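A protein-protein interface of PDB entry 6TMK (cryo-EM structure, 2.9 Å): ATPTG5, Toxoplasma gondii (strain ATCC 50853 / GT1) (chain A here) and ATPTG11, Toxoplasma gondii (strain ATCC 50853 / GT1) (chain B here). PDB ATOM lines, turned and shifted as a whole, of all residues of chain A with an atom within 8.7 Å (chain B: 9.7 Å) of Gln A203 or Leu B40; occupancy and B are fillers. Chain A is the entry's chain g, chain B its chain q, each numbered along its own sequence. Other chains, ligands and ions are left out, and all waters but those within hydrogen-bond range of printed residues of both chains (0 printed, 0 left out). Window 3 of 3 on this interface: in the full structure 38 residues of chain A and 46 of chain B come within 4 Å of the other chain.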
ATOM      1  N   ALA A 196     -26.158  16.734 -33.186  1.00  0.00           N
ATOM      2  CA  ALA A 196     -25.996  16.644 -31.741  1.00  0.00           C
ATOM      3  C   ALA A 196     -24.567  16.284 -31.364  1.00  0.00           C
ATOM      4  O   ALA A 196     -24.017  16.830 -30.400  1.00  0.00           O
ATOM      5  CB  ALA A 196     -26.970  15.617 -31.176  1.00  0.00           C
ATOM      6  N   ALA A 197     -23.953  15.362 -32.104  1.00  0.00           N
ATOM      7  CA  ALA A 197     -22.559  15.025 -31.847  1.00  0.00           C
ATOM      8  C   ALA A 197     -21.655  16.234 -32.034  1.00  0.00           C
ATOM      9  O   ALA A 197     -20.723  16.449 -31.252  1.00  0.00           O
ATOM     10  CB  ALA A 197     -22.125  13.884 -32.759  1.00  0.00           C
ATOM     11  N   ILE A 198     -21.914  17.038 -33.065  1.00  0.00           N
ATOM     12  CA  ILE A 198     -21.071  18.202 -33.311  1.00  0.00           C
ATOM     13  C   ILE A 198     -21.279  19.250 -32.229  1.00  0.00           C
ATOM     14  O   ILE A 198     -20.337  19.940 -31.826  1.00  0.00           O
ATOM     15  CB  ILE A 198     -21.336  18.760 -34.718  1.00  0.00           C
ATOM     16  CG1 ILE A 198     -20.748  17.801 -35.753  1.00  0.00           C
ATOM     17  CG2 ILE A 198     -20.767  20.157 -34.845  1.00  0.00           C
ATOM     18  CD1 ILE A 198     -21.007  18.166 -37.183  1.00  0.00           C
ATOM     19  N   ALA A 199     -22.509  19.382 -31.735  1.00  0.00           N
ATOM     20  CA  ALA A 199     -22.758  20.257 -30.595  1.00  0.00           C
ATOM     21  C   ALA A 199     -21.965  19.798 -29.379  1.00  0.00           C
ATOM     22  O   ALA A 199     -21.308  20.602 -28.704  1.00  0.00           O
ATOM     23  CB  ALA A 199     -24.251  20.292 -30.285  1.00  0.00           C
ATOM     24  N   CYS A 200     -22.012  18.497 -29.091  1.00  0.00           N
ATOM     25  CA  CYS A 200     -21.260  17.958 -27.965  1.00  0.00           C
ATOM     26  C   CYS A 200     -19.772  18.219 -28.129  1.00  0.00           C
ATOM     27  O   CYS A 200     -19.089  18.567 -27.163  1.00  0.00           O
ATOM     28  CB  CYS A 200     -21.523  16.458 -27.826  1.00  0.00           C
ATOM     29  SG  CYS A 200     -20.401  15.605 -26.692  1.00  0.00           S
ATOM     30  N   LEU A 201     -19.251  18.052 -29.340  1.00  0.00           N
ATOM     31  CA  LEU A 201     -17.826  18.261 -29.569  1.00  0.00           C
ATOM     32  C   LEU A 201     -17.450  19.726 -29.381  1.00  0.00           C
ATOM     33  O   LEU A 201     -16.455  20.046 -28.717  1.00  0.00           O
ATOM     34  CB  LEU A 201     -17.455  17.786 -30.969  1.00  0.00           C
ATOM     35  CG  LEU A 201     -17.572  16.283 -31.190  1.00  0.00           C
ATOM     36  CD1 LEU A 201     -17.629  15.964 -32.657  1.00  0.00           C
ATOM     37  CD2 LEU A 201     -16.417  15.569 -30.549  1.00  0.00           C
ATOM     38  N   SER A 202     -18.244  20.631 -29.955  1.00  0.00           N
ATOM     39  CA  SER A 202     -17.984  22.056 -29.810  1.00  0.00           C
ATOM     40  C   SER A 202     -18.035  22.489 -28.354  1.00  0.00           C
ATOM     41  O   SER A 202     -17.298  23.395 -27.952  1.00  0.00           O
ATOM     42  CB  SER A 202     -18.998  22.848 -30.627  1.00  0.00           C
ATOM     43  OG  SER A 202     -19.044  22.397 -31.966  1.00  0.00           O
ATOM     44  N   GLN A 203     -18.890  21.858 -27.552  1.00  0.00           N
ATOM     45  CA  GLN A 203     -18.983  22.238 -26.149  1.00  0.00           C
ATOM     46  C   GLN A 203     -17.870  21.606 -25.321  1.00  0.00           C
ATOM     47  O   GLN A 203     -17.341  22.243 -24.403  1.00  0.00           O
ATOM     48  CB  GLN A 203     -20.352  21.851 -25.594  1.00  0.00           C
ATOM     49  CG  GLN A 203     -21.493  22.677 -26.141  1.00  0.00           C
ATOM     50  CD  GLN A 203     -21.739  23.926 -25.328  1.00  0.00           C
ATOM     51  OE1 GLN A 203     -22.681  23.992 -24.539  1.00  0.00           O
ATOM     52  NE2 GLN A 203     -20.883  24.922 -25.504  1.00  0.00           N
ATOM     53  N   ARG A 204     -17.494  20.365 -25.631  1.00  0.00           N
ATOM     54  CA  ARG A 204     -16.619  19.571 -24.781  1.00  0.00           C
ATOM     55  C   ARG A 204     -15.235  19.378 -25.390  1.00  0.00           C
ATOM     56  O   ARG A 204     -14.546  18.409 -25.056  1.00  0.00           O
ATOM     57  CB  ARG A 204     -17.248  18.205 -24.507  1.00  0.00           C
ATOM     58  CG  ARG A 204     -18.736  18.216 -24.207  1.00  0.00           C
ATOM     59  CD  ARG A 204     -19.043  18.654 -22.799  1.00  0.00           C
ATOM     60  NE  ARG A 204     -20.465  18.932 -22.635  1.00  0.00           N
ATOM     61  CZ  ARG A 204     -21.087  19.001 -21.463  1.00  0.00           C
ATOM     62  NH1 ARG A 204     -20.416  18.815 -20.335  1.00  0.00           N
ATOM     63  NH2 ARG A 204     -22.386  19.260 -21.421  1.00  0.00           N
ATOM     64  N   GLU A 205     -14.814  20.273 -26.281  1.00  0.00           N
ATOM     65  CA  GLU A 205     -13.415  20.341 -26.705  1.00  0.00           C
ATOM     66  C   GLU A 205     -13.017  19.105 -27.514  1.00  0.00           C
ATOM     67  O   GLU A 205     -11.992  18.474 -27.258  1.00  0.00           O
ATOM     68  CB  GLU A 205     -12.489  20.517 -25.499  1.00  0.00           C
ATOM     69  CG  GLU A 205     -12.841  21.691 -24.600  1.00  0.00           C
ATOM     70  CD  GLU A 205     -12.306  23.011 -25.121  1.00  0.00           C
ATOM     71  OE1 GLU A 205     -11.132  23.050 -25.546  1.00  0.00           O
ATOM     72  OE2 GLU A 205     -13.057  24.008 -25.107  1.00  0.00           O
ATOM     73  N   GLY A 206     -13.840  18.766 -28.501  1.00  0.00           N
ATOM     74  CA  GLY A 206     -13.532  17.667 -29.388  1.00  0.00           C
ATOM     75  C   GLY A 206     -13.777  16.287 -28.831  1.00  0.00           C
ATOM     76  O   GLY A 206     -13.306  15.309 -29.422  1.00  0.00           O
ATOM     77  N   GLY A 207     -14.491  16.168 -27.717  1.00  0.00           N
ATOM     78  CA  GLY A 207     -14.763  14.861 -27.157  1.00  0.00           C
ATOM     79  C   GLY A 207     -13.618  14.278 -26.370  1.00  0.00           C
ATOM     80  O   GLY A 207     -13.489  13.053 -26.287  1.00  0.00           O
ATOM     81  N   LYS A 208     -12.781  15.126 -25.786  1.00  0.00           N
ATOM     82  CA  LYS A 208     -11.717  14.657 -24.914  1.00  0.00           C
ATOM     83  C   LYS A 208     -12.291  13.863 -23.746  1.00  0.00           C
ATOM     84  O   LYS A 208     -13.449  14.033 -23.359  1.00  0.00           O
ATOM     85  CB  LYS A 208     -10.898  15.837 -24.403  1.00  0.00           C
ATOM     86  CG  LYS A 208      -9.543  15.454 -23.852  1.00  0.00           C
ATOM     87  CD  LYS A 208      -8.513  16.532 -24.131  1.00  0.00           C
ATOM     88  CE  LYS A 208      -8.907  17.863 -23.505  1.00  0.00           C
ATOM     89  NZ  LYS A 208      -9.201  17.744 -22.051  1.00  0.00           N
ATOM     90  N   GLN A 211     -16.424  12.274 -23.862  1.00  0.00           N
ATOM     91  CA  GLN A 211     -17.558  13.129 -23.541  1.00  0.00           C
ATOM     92  C   GLN A 211     -18.653  13.127 -24.598  1.00  0.00           C
ATOM     93  O   GLN A 211     -19.762  13.581 -24.308  1.00  0.00           O
ATOM     94  CB  GLN A 211     -17.087  14.569 -23.308  1.00  0.00           C
ATOM     95  CG  GLN A 211     -16.274  14.730 -22.041  1.00  0.00           C
ATOM     96  CD  GLN A 211     -15.714  16.123 -21.870  1.00  0.00           C
ATOM     97  OE1 GLN A 211     -16.418  17.043 -21.453  1.00  0.00           O
ATOM     98  NE2 GLN A 211     -14.437  16.288 -22.186  1.00  0.00           N
ATOM     99  N   CYS A 212     -18.377  12.632 -25.805  1.00  0.00           N
ATOM    100  CA  CYS A 212     -19.389  12.473 -26.842  1.00  0.00           C
ATOM    101  C   CYS A 212     -19.624  11.002 -27.175  1.00  0.00           C
ATOM    102  O   CYS A 212     -20.201  10.677 -28.226  1.00  0.00           O
ATOM    103  CB  CYS A 212     -18.977  13.252 -28.090  1.00  0.00           C
ATOM    104  SG  CYS A 212     -18.809  15.049 -27.827  1.00  0.00           S
ATOM    105  N   PRO B  36     -27.095  11.358 -21.365  1.00  0.00           N
ATOM    106  CA  PRO B  36     -26.160  12.265 -22.025  1.00  0.00           C
ATOM    107  C   PRO B  36     -25.333  13.022 -21.004  1.00  0.00           C
ATOM    108  O   PRO B  36     -25.546  12.879 -19.790  1.00  0.00           O
ATOM    109  CB  PRO B  36     -27.075  13.215 -22.814  1.00  0.00           C
ATOM    110  CG  PRO B  36     -28.466  12.669 -22.660  1.00  0.00           C
ATOM    111  CD  PRO B  36     -28.462  11.896 -21.397  1.00  0.00           C
ATOM    112  N   PRO B  37     -24.379  13.835 -21.447  1.00  0.00           N
ATOM    113  CA  PRO B  37     -23.668  14.708 -20.511  1.00  0.00           C
ATOM    114  C   PRO B  37     -24.555  15.840 -20.022  1.00  0.00           C
ATOM    115  O   PRO B  37     -25.442  16.320 -20.732  1.00  0.00           O
ATOM    116  CB  PRO B  37     -22.485  15.239 -21.332  1.00  0.00           C
ATOM    117  CG  PRO B  37     -22.560  14.570 -22.673  1.00  0.00           C
ATOM    118  CD  PRO B  37     -23.935  14.031 -22.834  1.00  0.00           C
ATOM    119  N   ALA B  38     -24.306  16.265 -18.789  1.00  0.00           N
ATOM    120  CA  ALA B  38     -25.085  17.349 -18.218  1.00  0.00           C
ATOM    121  C   ALA B  38     -24.692  18.669 -18.877  1.00  0.00           C
ATOM    122  O   ALA B  38     -23.521  18.871 -19.212  1.00  0.00           O
ATOM    123  CB  ALA B  38     -24.868  17.435 -16.710  1.00  0.00           C
ATOM    124  N   PRO B  39     -25.636  19.590 -19.074  1.00  0.00           N
ATOM    125  CA  PRO B  39     -25.289  20.870 -19.710  1.00  0.00           C
ATOM    126  C   PRO B  39     -24.342  21.667 -18.825  1.00  0.00           C
ATOM    127  O   PRO B  39     -24.672  22.009 -17.688  1.00  0.00           O
ATOM    128  CB  PRO B  39     -26.645  21.567 -19.870  1.00  0.00           C
ATOM    129  CG  PRO B  39     -27.510  20.947 -18.829  1.00  0.00           C
ATOM    130  CD  PRO B  39     -27.066  19.520 -18.733  1.00  0.00           C
ATOM    131  N   LEU B  40     -23.159  21.957 -19.356  1.00  0.00           N
ATOM    132  CA  LEU B  40     -22.148  22.670 -18.598  1.00  0.00           C
ATOM    133  C   LEU B  40     -22.601  24.101 -18.310  1.00  0.00           C
ATOM    134  O   LEU B  40     -23.445  24.653 -19.019  1.00  0.00           O
ATOM    135  CB  LEU B  40     -20.827  22.668 -19.362  1.00  0.00           C
ATOM    136  CG  LEU B  40     -20.658  23.665 -20.509  1.00  0.00           C
ATOM    137  CD1 LEU B  40     -19.244  23.587 -21.054  1.00  0.00           C
ATOM    138  CD2 LEU B  40     -21.672  23.405 -21.605  1.00  0.00           C
ATOM    139  N   PRO B  41     -22.049  24.725 -17.269  1.00  0.00           N
ATOM    140  CA  PRO B  41     -22.433  26.106 -16.953  1.00  0.00           C
ATOM    141  C   PRO B  41     -22.044  27.055 -18.076  1.00  0.00           C
ATOM    142  O   PRO B  41     -20.925  27.007 -18.592  1.00  0.00           O
ATOM    143  CB  PRO B  41     -21.657  26.401 -15.664  1.00  0.00           C
ATOM    144  CG  PRO B  41     -20.497  25.468 -15.711  1.00  0.00           C
ATOM    145  CD  PRO B  41     -21.043  24.215 -16.323  1.00  0.00           C
ATOM    146  N   SER B  42     -22.977  27.920 -18.454  1.00  0.00           N
ATOM    147  CA  SER B  42     -22.746  28.781 -19.601  1.00  0.00           C
ATOM    148  C   SER B  42     -21.615  29.763 -19.298  1.00  0.00           C
ATOM    149  O   SER B  42     -21.555  30.324 -18.200  1.00  0.00           O
ATOM    150  CB  SER B  42     -24.017  29.544 -19.962  1.00  0.00           C
ATOM    151  OG  SER B  42     -23.760  30.518 -20.959  1.00  0.00           O
ATOM    152  N   PRO B  43     -20.704  29.990 -20.248  1.00  0.00           N
ATOM    153  CA  PRO B  43     -19.508  30.785 -19.949  1.00  0.00           C
ATOM    154  C   PRO B  43     -19.715  32.276 -20.149  1.00  0.00           C
ATOM    155  O   PRO B  43     -20.811  32.721 -20.504  1.00  0.00           O
ATOM    156  CB  PRO B  43     -18.486  30.225 -20.938  1.00  0.00           C
ATOM    157  CG  PRO B  43     -19.313  29.944 -22.140  1.00  0.00           C
ATOM    158  CD  PRO B  43     -20.658  29.463 -21.624  1.00  0.00           C
ATOM    159  N   SER B  44     -18.663  33.055 -19.923  1.00  0.00           N
ATOM    160  CA  SER B  44     -18.652  34.473 -20.260  1.00  0.00           C
ATOM    161  C   SER B  44     -17.204  34.948 -20.205  1.00  0.00           C
ATOM    162  O   SER B  44     -16.287  34.172 -19.920  1.00  0.00           O
ATOM    163  CB  SER B  44     -19.547  35.276 -19.316  1.00  0.00           C
ATOM    164  OG  SER B  44     -20.916  35.028 -19.583  1.00  0.00           O
ATOM    165  N   GLN B  47     -13.722  34.910 -17.425  1.00  0.00           N
ATOM    166  CA  GLN B  47     -12.735  33.877 -17.149  1.00  0.00           C
ATOM    167  C   GLN B  47     -11.497  33.955 -18.032  1.00  0.00           C
ATOM    168  O   GLN B  47     -10.629  33.083 -17.924  1.00  0.00           O
ATOM    169  CB  GLN B  47     -13.380  32.498 -17.308  1.00  0.00           C
ATOM    170  CG  GLN B  47     -14.714  32.360 -16.600  1.00  0.00           C
ATOM    171  CD  GLN B  47     -15.249  30.945 -16.631  1.00  0.00           C
ATOM    172  OE1 GLN B  47     -14.538  30.007 -16.987  1.00  0.00           O
ATOM    173  NE2 GLN B  47     -16.515  30.786 -16.267  1.00  0.00           N
ATOM    174  N   LYS B  81      -9.594  30.214 -27.616  1.00  0.00           N
ATOM    175  CA  LYS B  81     -10.482  29.155 -27.155  1.00  0.00           C
ATOM    176  C   LYS B  81     -11.467  29.687 -26.125  1.00  0.00           C
ATOM    177  O   LYS B  81     -12.662  29.360 -26.161  1.00  0.00           O
ATOM    178  CB  LYS B  81      -9.661  28.016 -26.567  1.00  0.00           C
ATOM    179  CG  LYS B  81      -9.175  27.017 -27.589  1.00  0.00           C
ATOM    180  CD  LYS B  81      -8.793  25.706 -26.938  1.00  0.00           C
ATOM    181  CE  LYS B  81      -7.794  25.928 -25.822  1.00  0.00           C
ATOM    182  NZ  LYS B  81      -6.916  24.750 -25.607  1.00  0.00           N
ATOM    183  N   PHE B  83     -12.602  32.696 -25.809  1.00  0.00           N
ATOM    184  CA  PHE B  83     -13.623  33.494 -26.497  1.00  0.00           C
ATOM    185  C   PHE B  83     -14.584  32.614 -27.298  1.00  0.00           C
ATOM    186  O   PHE B  83     -15.800  32.871 -27.348  1.00  0.00           O
ATOM    187  CB  PHE B  83     -12.954  34.521 -27.405  1.00  0.00           C
ATOM    188  CG  PHE B  83     -12.410  35.711 -26.673  1.00  0.00           C
ATOM    189  CD1 PHE B  83     -13.259  36.695 -26.202  1.00  0.00           C
ATOM    190  CD2 PHE B  83     -11.053  35.844 -26.453  1.00  0.00           C
ATOM    191  CE1 PHE B  83     -12.762  37.790 -25.529  1.00  0.00           C
ATOM    192  CE2 PHE B  83     -10.553  36.937 -25.781  1.00  0.00           C
ATOM    193  CZ  PHE B  83     -11.409  37.909 -25.316  1.00  0.00           C
ATOM    194  N   ARG B  84     -14.051  31.590 -27.958  1.00  0.00           N
ATOM    195  CA  ARG B  84     -14.883  30.735 -28.787  1.00  0.00           C
ATOM    196  C   ARG B  84     -15.889  29.971 -27.946  1.00  0.00           C
ATOM    197  O   ARG B  84     -16.973  29.637 -28.432  1.00  0.00           O
ATOM    198  CB  ARG B  84     -14.004  29.775 -29.583  1.00  0.00           C
ATOM    199  CG  ARG B  84     -13.324  30.413 -30.774  1.00  0.00           C
ATOM    200  CD  ARG B  84     -12.476  29.410 -31.522  1.00  0.00           C
ATOM    201  NE  ARG B  84     -11.141  29.921 -31.820  1.00  0.00           N
ATOM    202  CZ  ARG B  84     -10.003  29.297 -31.527  1.00  0.00           C
ATOM    203  NH1 ARG B  84     -10.000  28.124 -30.911  1.00  0.00           N
ATOM    204  NH2 ARG B  84      -8.849  29.856 -31.849  1.00  0.00           N
ATOM    205  N   ARG B  85     -15.551  29.690 -26.688  1.00  0.00           N
ATOM    206  CA  ARG B  85     -16.528  29.108 -25.774  1.00  0.00           C
ATOM    207  C   ARG B  85     -17.813  29.929 -25.741  1.00  0.00           C
ATOM    208  O   ARG B  85     -18.913  29.396 -25.937  1.00  0.00           O
ATOM    209  CB  ARG B  85     -15.926  29.006 -24.376  1.00  0.00           C
ATOM    210  CG  ARG B  85     -15.276  27.677 -24.082  1.00  0.00           C
ATOM    211  CD  ARG B  85     -14.513  27.719 -22.779  1.00  0.00           C
ATOM    212  NE  ARG B  85     -15.396  27.899 -21.633  1.00  0.00           N
ATOM    213  CZ  ARG B  85     -14.977  28.043 -20.380  1.00  0.00           C
ATOM    214  NH1 ARG B  85     -13.679  28.033 -20.104  1.00  0.00           N
ATOM    215  NH2 ARG B  85     -15.855  28.201 -19.401  1.00  0.00           N
ATOM    216  N   VAL B  86     -17.689  31.239 -25.527  1.00  0.00           N
ATOM    217  CA  VAL B  86     -18.878  32.070 -25.368  1.00  0.00           C
ATOM    218  C   VAL B  86     -19.573  32.254 -26.707  1.00  0.00           C
ATOM    219  O   VAL B  86     -20.809  32.294 -26.781  1.00  0.00           O
ATOM    220  CB  VAL B  86     -18.525  33.418 -24.713  1.00  0.00           C
ATOM    221  CG1 VAL B  86     -17.859  33.192 -23.369  1.00  0.00           C
ATOM    222  CG2 VAL B  86     -17.627  34.253 -25.596  1.00  0.00           C
ATOM    223  N   SER B  87     -18.800  32.350 -27.792  1.00  0.00           N
ATOM    224  CA  SER B  87     -19.443  32.488 -29.097  1.00  0.00           C
ATOM    225  C   SER B  87     -20.267  31.248 -29.428  1.00  0.00           C
ATOM    226  O   SER B  87     -21.402  31.352 -29.916  1.00  0.00           O
ATOM    227  CB  SER B  87     -18.394  32.738 -30.175  1.00  0.00           C
ATOM    228  OG  SER B  87     -17.589  31.592 -30.362  1.00  0.00           O
ATOM    229  N   VAL B  88     -19.725  30.065 -29.139  1.00  0.00           N
ATOM    230  CA  VAL B  88     -20.446  28.828 -29.406  1.00  0.00           C
ATOM    231  C   VAL B  88     -21.665  28.719 -28.503  1.00  0.00           C
ATOM    232  O   VAL B  88     -22.721  28.232 -28.923  1.00  0.00           O
ATOM    233  CB  VAL B  88     -19.510  27.623 -29.232  1.00  0.00           C
ATOM    234  CG1 VAL B  88     -20.301  26.342 -29.235  1.00  0.00           C
ATOM    235  CG2 VAL B  88     -18.478  27.605 -30.327  1.00  0.00           C
ATOM    236  N   ALA B  89     -21.536  29.143 -27.245  1.00  0.00           N
ATOM    237  CA  ALA B  89     -22.685  29.108 -26.349  1.00  0.00           C
ATOM    238  C   ALA B  89     -23.812  29.980 -26.884  1.00  0.00           C
ATOM    239  O   ALA B  89     -24.981  29.574 -26.880  1.00  0.00           O
ATOM    240  CB  ALA B  89     -22.272  29.559 -24.951  1.00  0.00           C
ATOM    241  N   GLU B  90     -23.473  31.179 -27.361  1.00  0.00           N
ATOM    242  CA  GLU B  90     -24.486  32.058 -27.929  1.00  0.00           C
ATOM    243  C   GLU B  90     -25.138  31.424 -29.149  1.00  0.00           C
ATOM    244  O   GLU B  90     -26.366  31.450 -29.293  1.00  0.00           O
ATOM    245  CB  GLU B  90     -23.862  33.401 -28.300  1.00  0.00           C
ATOM    246  CG  GLU B  90     -24.871  34.450 -28.741  1.00  0.00           C
ATOM    247  CD  GLU B  90     -24.889  34.651 -30.245  1.00  0.00           C
ATOM    248  OE1 GLU B  90     -23.806  34.624 -30.867  1.00  0.00           O
ATOM    249  OE2 GLU B  90     -25.989  34.835 -30.807  1.00  0.00           O
ATOM    250  N   VAL B  91     -24.332  30.828 -30.028  1.00  0.00           N
ATOM    251  CA  VAL B  91     -24.883  30.205 -31.228  1.00  0.00           C
ATOM    252  C   VAL B  91     -25.853  29.093 -30.851  1.00  0.00           C
ATOM    253  O   VAL B  91     -26.979  29.022 -31.361  1.00  0.00           O
ATOM    254  CB  VAL B  91     -23.751  29.677 -32.124  1.00  0.00           C
ATOM    255  CG1 VAL B  91     -24.292  28.678 -33.118  1.00  0.00           C
ATOM    256  CG2 VAL B  91     -23.073  30.820 -32.845  1.00  0.00           C
ATOM    257  N   LEU B  92     -25.433  28.218 -29.937  1.00  0.00           N
ATOM    258  CA  LEU B  92     -26.262  27.083 -29.549  1.00  0.00           C
ATOM    259  C   LEU B  92     -27.562  27.547 -28.907  1.00  0.00           C
ATOM    260  O   LEU B  92     -28.640  27.034 -29.225  1.00  0.00           O
ATOM    261  CB  LEU B  92     -25.494  26.175 -28.590  1.00  0.00           C
ATOM    262  CG  LEU B  92     -24.306  25.407 -29.163  1.00  0.00           C
ATOM    263  CD1 LEU B  92     -23.607  24.635 -28.067  1.00  0.00           C
ATOM    264  CD2 LEU B  92     -24.750  24.473 -30.263  1.00  0.00           C
ATOM    265  N   GLU B  93     -27.484  28.518 -27.995  1.00  0.00           N
ATOM    266  CA  GLU B  93     -28.689  28.926 -27.286  1.00  0.00           C
ATOM    267  C   GLU B  93     -29.638  29.696 -28.194  1.00  0.00           C
ATOM    268  O   GLU B  93     -30.856  29.637 -27.998  1.00  0.00           O
ATOM    269  CB  GLU B  93     -28.331  29.759 -26.054  1.00  0.00           C
ATOM    270  CG  GLU B  93     -27.675  31.094 -26.356  1.00  0.00           C
ATOM    271  CD  GLU B  93     -28.677  32.212 -26.585  1.00  0.00           C
ATOM    272  OE1 GLU B  93     -29.892  31.974 -26.420  1.00  0.00           O
ATOM    273  OE2 GLU B  93     -28.248  33.334 -26.929  1.00  0.00           O
ATOM    274  N   PHE B  98     -30.472  24.010 -33.370  1.00  0.00           N
ATOM    275  CA  PHE B  98     -29.739  23.254 -32.367  1.00  0.00           C
ATOM    276  C   PHE B  98     -30.533  23.008 -31.092  1.00  0.00           C
ATOM    277  O   PHE B  98     -30.028  22.337 -30.191  1.00  0.00           O
ATOM    278  CB  PHE B  98     -28.441  23.981 -32.022  1.00  0.00           C
ATOM    279  CG  PHE B  98     -27.467  24.045 -33.157  1.00  0.00           C
ATOM    280  CD1 PHE B  98     -26.686  22.952 -33.474  1.00  0.00           C
ATOM    281  CD2 PHE B  98     -27.339  25.193 -33.910  1.00  0.00           C
ATOM    282  CE1 PHE B  98     -25.793  23.007 -34.518  1.00  0.00           C
ATOM    283  CE2 PHE B  98     -26.447  25.253 -34.953  1.00  0.00           C
ATOM    284  CZ  PHE B  98     -25.674  24.158 -35.258  1.00  0.00           C
ATOM    285  N   ALA B 101     -31.126  19.479 -30.935  1.00  0.00           N
ATOM    286  CA  ALA B 101     -29.928  18.690 -30.735  1.00  0.00           C
ATOM    287  C   ALA B 101     -29.514  18.785 -29.282  1.00  0.00           C
ATOM    288  O   ALA B 101     -29.000  17.814 -28.714  1.00  0.00           O
ATOM    289  CB  ALA B 101     -28.814  19.177 -31.656  1.00  0.00           C
ATOM    290  N   ARG B 102     -29.727  19.948 -28.666  1.00  0.00           N
ATOM    291  CA  ARG B 102     -29.409  20.079 -27.255  1.00  0.00           C
ATOM    292  C   ARG B 102     -30.300  19.143 -26.459  1.00  0.00           C
ATOM    293  O   ARG B 102     -29.823  18.386 -25.606  1.00  0.00           O
ATOM    294  CB  ARG B 102     -29.584  21.524 -26.789  1.00  0.00           C
ATOM    295  CG  ARG B 102     -28.351  22.390 -26.977  1.00  0.00           C
ATOM    296  CD  ARG B 102     -28.483  23.714 -26.239  1.00  0.00           C
ATOM    297  NE  ARG B 102     -29.691  24.446 -26.605  1.00  0.00           N
ATOM    298  CZ  ARG B 102     -30.049  25.610 -26.069  1.00  0.00           C
ATOM    299  NH1 ARG B 102     -29.292  26.178 -25.139  1.00  0.00           N
ATOM    300  NH2 ARG B 102     -31.166  26.205 -26.460  1.00  0.00           N
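The guanidinium group (NH2) of Arg A204 sits at hydrogen-bond distance from the backbone carbonyl oxygen (O) of Ala B38 (2.5 Å). NH2 of Arg A204 sits close to N of Leu B40, 3.5 Å away.
OG of Ser A202 is in hydrogen-bond range of O of Ile A198 (2.8 Å). The backbone carbonyl oxygen (O) of Lys A208 lies within hydrogen-bond range of the side-chain amide nitrogen (NE2) of Gln A211 (2.7 Å). The side-chain sulfur (SG) of Cys A200 forms a disulfide with the side-chain sulfur (SG) of Cys A212 (2.0 Å).
Ala B101 touches Ala A196. Ser A202 touches Val B88 (CB to CG1, 3.98 Å). Leu B40 touches Gln A203 (CD2 to OE1, 3.2 Å). CD of Gln A203 touches CD1 of Leu B92 (3.4 Å). Pro B39 touches Arg A204. Glu A205 touches Lys B81 (OE1 to CD, 3.8 Å). Gln A211 touches Pro B37 (O to CG, 3.4 Å).
Of chain A, only Gln A203 (3.2 Å) and Arg A204 (3.5 Å) come within 4 Å of Leu B40. Of chain A, only Arg A204 comes within 4 Å of Pro B39. No residue of chain A comes within 4 Å of Pro B41. Of the printed residues of chain A, Leu B92 touches Gln A203 (3.4 Å). Of the printed residues of chain A, Lys B81 touches Glu A205 (3.8 Å). Of the printed residues of chain A, Val B88 touches Ser A202. Of the printed residues of chain A, Pro B37 touches Gln A211. Of the printed residues of chain A, Ala B101 touches Ala A196 (3.8 Å). Phe B98 touches none of the printed residues of chain A. Ala A199 touches none of the printed residues of chain B. The nearest residue of chain B that does not touch Gln A203 is Val B88 (4.03 Å). The nearest residue of chain A that does not touch Leu B40 is Gln A211 (7.1 Å). The nearest printed residue of chain A that does not touch Pro B37 is Arg A204 (4.02 Å).
Of the 25 printed residues of chain B, 8 touch a printed residue of chain A. Among the printed residues, no Asp or Glu carboxylate lies within 4 Å of a Lys or Arg side-chain nitrogen of the other chain.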
